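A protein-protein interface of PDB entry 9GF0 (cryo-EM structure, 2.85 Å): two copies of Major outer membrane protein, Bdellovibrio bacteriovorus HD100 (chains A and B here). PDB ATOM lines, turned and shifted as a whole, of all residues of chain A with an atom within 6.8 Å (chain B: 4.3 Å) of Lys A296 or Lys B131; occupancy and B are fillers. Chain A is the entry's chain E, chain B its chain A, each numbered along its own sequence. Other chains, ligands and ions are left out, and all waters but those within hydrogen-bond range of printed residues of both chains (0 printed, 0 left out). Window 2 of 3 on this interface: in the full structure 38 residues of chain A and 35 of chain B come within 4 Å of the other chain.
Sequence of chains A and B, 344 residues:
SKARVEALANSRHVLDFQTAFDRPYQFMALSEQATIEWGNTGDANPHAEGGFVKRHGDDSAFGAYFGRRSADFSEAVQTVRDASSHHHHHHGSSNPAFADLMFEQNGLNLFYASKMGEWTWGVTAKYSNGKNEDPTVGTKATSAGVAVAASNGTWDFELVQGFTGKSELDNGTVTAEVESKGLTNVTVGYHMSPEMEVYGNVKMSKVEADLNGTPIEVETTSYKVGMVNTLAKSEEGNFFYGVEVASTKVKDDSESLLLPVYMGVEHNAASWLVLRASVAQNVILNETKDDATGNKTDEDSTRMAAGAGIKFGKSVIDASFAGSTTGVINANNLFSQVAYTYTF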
ATOM      1  N   GLU A 287     -16.575 -26.356  -1.439  1.00  0.00           N
ATOM      2  CA  GLU A 287     -16.161 -25.960  -0.072  1.00  0.00           C
ATOM      3  C   GLU A 287     -17.335 -25.686   0.860  1.00  0.00           C
ATOM      4  O   GLU A 287     -18.195 -24.883   0.498  1.00  0.00           O
ATOM      5  CB  GLU A 287     -15.358 -24.669  -0.164  1.00  0.00           C
ATOM      6  CG  GLU A 287     -14.299 -24.521   0.902  1.00  0.00           C
ATOM      7  CD  GLU A 287     -13.445 -23.289   0.669  1.00  0.00           C
ATOM      8  OE1 GLU A 287     -12.259 -23.452   0.338  1.00  0.00           O
ATOM      9  OE2 GLU A 287     -13.980 -22.172   0.796  1.00  0.00           O
ATOM     10  N   THR A 288     -17.312 -26.285   2.043  1.00  0.00           N
ATOM     11  CA  THR A 288     -18.331 -26.044   3.065  1.00  0.00           C
ATOM     12  C   THR A 288     -17.630 -25.478   4.298  1.00  0.00           C
ATOM     13  O   THR A 288     -17.257 -26.218   5.210  1.00  0.00           O
ATOM     14  CB  THR A 288     -19.107 -27.316   3.406  1.00  0.00           C
ATOM     15  OG1 THR A 288     -18.336 -28.125   4.300  1.00  0.00           O
ATOM     16  CG2 THR A 288     -19.402 -28.111   2.150  1.00  0.00           C
ATOM     17  N   LYS A 289     -17.461 -24.160   4.320  1.00  0.00           N
ATOM     18  CA  LYS A 289     -16.805 -23.495   5.437  1.00  0.00           C
ATOM     19  C   LYS A 289     -17.649 -23.621   6.701  1.00  0.00           C
ATOM     20  O   LYS A 289     -18.874 -23.488   6.658  1.00  0.00           O
ATOM     21  CB  LYS A 289     -16.568 -22.026   5.096  1.00  0.00           C
ATOM     22  CG  LYS A 289     -16.241 -21.142   6.278  1.00  0.00           C
ATOM     23  CD  LYS A 289     -16.443 -19.679   5.925  1.00  0.00           C
ATOM     24  CE  LYS A 289     -15.254 -19.119   5.164  1.00  0.00           C
ATOM     25  NZ  LYS A 289     -13.970 -19.369   5.869  1.00  0.00           N
ATOM     26  N   ASP A 290     -16.994 -23.877   7.827  1.00  0.00           N
ATOM     27  CA  ASP A 290     -17.666 -24.020   9.112  1.00  0.00           C
ATOM     28  C   ASP A 290     -17.479 -22.741   9.915  1.00  0.00           C
ATOM     29  O   ASP A 290     -16.347 -22.310  10.150  1.00  0.00           O
ATOM     30  CB  ASP A 290     -17.120 -25.223   9.881  1.00  0.00           C
ATOM     31  CG  ASP A 290     -17.979 -25.592  11.071  1.00  0.00           C
ATOM     32  OD1 ASP A 290     -17.858 -24.929  12.120  1.00  0.00           O
ATOM     33  OD2 ASP A 290     -18.772 -26.549  10.957  1.00  0.00           O
ATOM     34  N   THR A 293     -15.119 -21.197  13.377  1.00  0.00           N
ATOM     35  CA  THR A 293     -13.798 -21.815  13.321  1.00  0.00           C
ATOM     36  C   THR A 293     -12.987 -21.363  12.117  1.00  0.00           C
ATOM     37  O   THR A 293     -11.777 -21.169  12.238  1.00  0.00           O
ATOM     38  CB  THR A 293     -13.920 -23.350  13.303  1.00  0.00           C
ATOM     39  OG1 THR A 293     -14.856 -23.746  12.294  1.00  0.00           O
ATOM     40  CG2 THR A 293     -14.385 -23.870  14.653  1.00  0.00           C
ATOM     41  N   GLY A 294     -13.627 -21.178  10.965  1.00  0.00           N
ATOM     42  CA  GLY A 294     -12.934 -20.850   9.740  1.00  0.00           C
ATOM     43  C   GLY A 294     -12.416 -22.039   8.962  1.00  0.00           C
ATOM     44  O   GLY A 294     -11.892 -21.852   7.857  1.00  0.00           O
ATOM     45  N   ASN A 295     -12.545 -23.250   9.495  1.00  0.00           N
ATOM     46  CA  ASN A 295     -12.033 -24.437   8.827  1.00  0.00           C
ATOM     47  C   ASN A 295     -12.968 -24.874   7.710  1.00  0.00           C
ATOM     48  O   ASN A 295     -14.187 -24.928   7.886  1.00  0.00           O
ATOM     49  CB  ASN A 295     -11.855 -25.578   9.827  1.00  0.00           C
ATOM     50  CG  ASN A 295     -11.042 -25.168  11.036  1.00  0.00           C
ATOM     51  OD1 ASN A 295     -10.080 -24.410  10.926  1.00  0.00           O
ATOM     52  ND2 ASN A 295     -11.421 -25.676  12.200  1.00  0.00           N
ATOM     53  N   LYS A 296     -12.386 -25.202   6.561  1.00  0.00           N
ATOM     54  CA  LYS A 296     -13.135 -25.646   5.399  1.00  0.00           C
ATOM     55  C   LYS A 296     -13.120 -27.168   5.317  1.00  0.00           C
ATOM     56  O   LYS A 296     -12.533 -27.860   6.148  1.00  0.00           O
ATOM     57  CB  LYS A 296     -12.565 -25.025   4.126  1.00  0.00           C
ATOM     58  CG  LYS A 296     -11.787 -23.750   4.353  1.00  0.00           C
ATOM     59  CD  LYS A 296     -12.652 -22.535   4.086  1.00  0.00           C
ATOM     60  CE  LYS A 296     -11.813 -21.353   3.636  1.00  0.00           C
ATOM     61  NZ  LYS A 296     -12.639 -20.298   2.984  1.00  0.00           N
ATOM     62  N   THR A 297     -13.787 -27.694   4.296  1.00  0.00           N
ATOM     63  CA  THR A 297     -13.841 -29.133   4.075  1.00  0.00           C
ATOM     64  C   THR A 297     -14.124 -29.372   2.602  1.00  0.00           C
ATOM     65  O   THR A 297     -15.149 -28.921   2.088  1.00  0.00           O
ATOM     66  CB  THR A 297     -14.909 -29.788   4.953  1.00  0.00           C
ATOM     67  OG1 THR A 297     -14.565 -29.613   6.332  1.00  0.00           O
ATOM     68  CG2 THR A 297     -15.008 -31.268   4.661  1.00  0.00           C
ATOM     69  N   ASP A 298     -13.209 -30.066   1.928  1.00  0.00           N
ATOM     70  CA  ASP A 298     -13.304 -30.362   0.498  1.00  0.00           C
ATOM     71  C   ASP A 298     -12.950 -31.832   0.294  1.00  0.00           C
ATOM     72  O   ASP A 298     -11.787 -32.171   0.070  1.00  0.00           O
ATOM     73  CB  ASP A 298     -12.388 -29.446  -0.303  1.00  0.00           C
ATOM     74  CG  ASP A 298     -12.882 -29.219  -1.707  1.00  0.00           C
ATOM     75  OD1 ASP A 298     -13.883 -29.856  -2.077  1.00  0.00           O
ATOM     76  OD2 ASP A 298     -12.275 -28.409  -2.440  1.00  0.00           O
ATOM     77  N   GLU A 299     -13.950 -32.701   0.367  1.00  0.00           N
ATOM     78  CA  GLU A 299     -13.745 -34.129   0.211  1.00  0.00           C
ATOM     79  C   GLU A 299     -14.212 -34.580  -1.168  1.00  0.00           C
ATOM     80  O   GLU A 299     -14.711 -33.794  -1.976  1.00  0.00           O
ATOM     81  CB  GLU A 299     -14.477 -34.896   1.309  1.00  0.00           C
ATOM     82  CG  GLU A 299     -14.443 -34.211   2.654  1.00  0.00           C
ATOM     83  CD  GLU A 299     -13.509 -34.892   3.630  1.00  0.00           C
ATOM     84  OE1 GLU A 299     -12.872 -35.895   3.245  1.00  0.00           O
ATOM     85  OE2 GLU A 299     -13.413 -34.426   4.783  1.00  0.00           O
ATOM     86  N   ASP A 300     -14.034 -35.867  -1.445  1.00  0.00           N
ATOM     87  CA  ASP A 300     -14.514 -36.428  -2.698  1.00  0.00           C
ATOM     88  C   ASP A 300     -16.035 -36.449  -2.714  1.00  0.00           C
ATOM     89  O   ASP A 300     -16.681 -36.746  -1.706  1.00  0.00           O
ATOM     90  CB  ASP A 300     -13.958 -37.834  -2.902  1.00  0.00           C
ATOM     91  CG  ASP A 300     -14.096 -38.313  -4.330  1.00  0.00           C
ATOM     92  OD1 ASP A 300     -13.312 -37.870  -5.194  1.00  0.00           O
ATOM     93  OD2 ASP A 300     -14.982 -39.150  -4.586  1.00  0.00           O
ATOM     94  N   MET B 102      -4.856 -38.692   2.465  1.00  0.00           N
ATOM     95  CA  MET B 102      -5.905 -38.435   1.493  1.00  0.00           C
ATOM     96  C   MET B 102      -5.535 -39.011   0.135  1.00  0.00           C
ATOM     97  O   MET B 102      -4.412 -38.836  -0.341  1.00  0.00           O
ATOM     98  CB  MET B 102      -6.142 -36.928   1.380  1.00  0.00           C
ATOM     99  CG  MET B 102      -7.374 -36.432   2.111  1.00  0.00           C
ATOM    100  SD  MET B 102      -8.009 -34.880   1.469  1.00  0.00           S
ATOM    101  CE  MET B 102      -9.665 -34.905   2.143  1.00  0.00           C
ATOM    102  N   GLY B 130      -8.278 -31.393  -2.839  1.00  0.00           N
ATOM    103  CA  GLY B 130      -9.149 -31.693  -1.688  1.00  0.00           C
ATOM    104  C   GLY B 130      -8.546 -31.211  -0.383  1.00  0.00           C
ATOM    105  O   GLY B 130      -7.408 -30.739  -0.415  1.00  0.00           O
ATOM    106  N   LYS B 131      -9.281 -31.328   0.724  1.00  0.00           N
ATOM    107  CA  LYS B 131      -8.805 -30.873   2.055  1.00  0.00           C
ATOM    108  C   LYS B 131      -9.787 -31.298   3.146  1.00  0.00           C
ATOM    109  O   LYS B 131     -10.828 -31.858   2.812  1.00  0.00           O
ATOM    110  CB  LYS B 131      -8.662 -29.353   2.100  1.00  0.00           C
ATOM    111  CG  LYS B 131      -9.942 -28.551   1.934  1.00  0.00           C
ATOM    112  CD  LYS B 131      -9.705 -27.063   2.016  1.00  0.00           C
ATOM    113  CE  LYS B 131     -10.972 -26.255   1.852  1.00  0.00           C
ATOM    114  NZ  LYS B 131     -10.716 -24.797   1.937  1.00  0.00           N
ATOM    115  N   ASN B 132      -9.440 -31.065   4.410  1.00  0.00           N
ATOM    116  CA  ASN B 132     -10.343 -31.355   5.553  1.00  0.00           C
ATOM    117  C   ASN B 132     -10.153 -30.223   6.551  1.00  0.00           C
ATOM    118  O   ASN B 132     -11.116 -29.933   7.251  1.00  0.00           O
ATOM    119  CB  ASN B 132     -10.058 -32.681   6.244  1.00  0.00           C
ATOM    120  CG  ASN B 132     -11.273 -33.334   6.864  1.00  0.00           C
ATOM    121  OD1 ASN B 132     -12.020 -32.698   7.603  1.00  0.00           O
ATOM    122  ND2 ASN B 132     -11.465 -34.611   6.585  1.00  0.00           N
ATOM    123  N   GLU B 133      -8.978 -29.598   6.570  1.00  0.00           N
ATOM    124  CA  GLU B 133      -8.720 -28.410   7.433  1.00  0.00           C
ATOM    125  C   GLU B 133      -9.330 -28.583   8.829  1.00  0.00           C
ATOM    126  O   GLU B 133      -9.259 -27.622   9.604  1.00  0.00           O
ATOM    127  CB  GLU B 133      -9.180 -27.126   6.750  1.00  0.00           C
ATOM    128  CG  GLU B 133      -8.073 -26.404   6.014  1.00  0.00           C
ATOM    129  CD  GLU B 133      -8.403 -24.968   5.646  1.00  0.00           C
ATOM    130  OE1 GLU B 133      -8.933 -24.245   6.511  1.00  0.00           O
ATOM    131  OE2 GLU B 133      -8.133 -24.577   4.495  1.00  0.00           O
ATOM    132  N   THR B 139      -5.842 -32.631   6.548  1.00  0.00           N
ATOM    133  CA  THR B 139      -5.347 -33.333   5.338  1.00  0.00           C
ATOM    134  C   THR B 139      -5.273 -32.368   4.154  1.00  0.00           C
ATOM    135  O   THR B 139      -5.758 -31.240   4.301  1.00  0.00           O
ATOM    136  CB  THR B 139      -6.202 -34.566   5.030  1.00  0.00           C
ATOM    137  OG1 THR B 139      -7.554 -34.138   4.891  1.00  0.00           O
ATOM    138  CG2 THR B 139      -6.102 -35.631   6.098  1.00  0.00           C
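Gly A294 touches none of the printed residues of chain B.
Lys A296 touches three residues of chain B.
Of the printed residues of chain B, Glu A299 touches Met B102 (3.5 Å) and Asn B132 (2.7 Å).
Of the printed residues of chain A, Met B102 touches Glu A299 (3.5 Å).
Of the printed residues of chain A, Lys B131 touches Glu A287 (2.6 Å), Lys A296 (2.8 Å), Thr A297 (3.996 Å) and Asp A298 (2.7 Å).
Of the printed residues of chain A, Asn B132 touches Lys A296, Thr A297 and Glu A299.
The nearest printed residue of chain B that does not touch Lys A296 is Thr B139 (7.8 Å).
The nearest printed residue of chain A that does not touch Lys B131 is Glu A299 (4.1 Å).
Among the printed residues, merely in contact across the chains: Lys A296 with Lys B131, Asp A298 with Gly B130, Asn A295 with Glu B133, Lys A296 with Glu B133, Glu A299 with Met B102, Thr A297 with Asn B132 and Thr A297 with Lys B131.
The side-chain amino group of Lys B131 is in salt-bridge range of the side-chain carboxylate of Glu A287 (2.6 Å).
O of Asp A298 is in hydrogen-bond range of N of Lys B131 (2.7 Å).
The backbone carbonyl oxygen of Asn B132 lies close to the backbone carbonyl oxygen of Lys A296, at 2.7 Å.
The side-chain amide nitrogen of Asn B132 sits at hydrogen-bond distance from the side-chain carboxylate of Glu A299, at 2.7 Å.
No position is printed for both chains.
Of the 11 pairs that touch across the chains among the printed residues, none has its exchanged pair printed and touching as well.
The side-chain sulfur (SD) of Met B102 lies within hydrogen-bond range of the side-chain hydroxyl (OG1) of Thr B139 (3.5 Å).
The side-chain amino group (NZ) of Lys B131 lies within salt-bridge range of the side-chain carboxylate (OE2) of Glu B133, at 3.6 Å.
OE2 of Glu A287 is in salt-bridge range of NZ of Lys A296 (3.2 Å).
The backbone NH (N) of Thr A288 is in hydrogen-bond range of the backbone carbonyl oxygen (O) of Thr A297 (3.4 Å).
The backbone NH (N) of Asp A290 is in hydrogen-bond range of the backbone carbonyl oxygen (O) of Asn A295, at 3.0 Å.
Of the 12 printed residues of chain A, 6 touch a printed residue of chain B.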
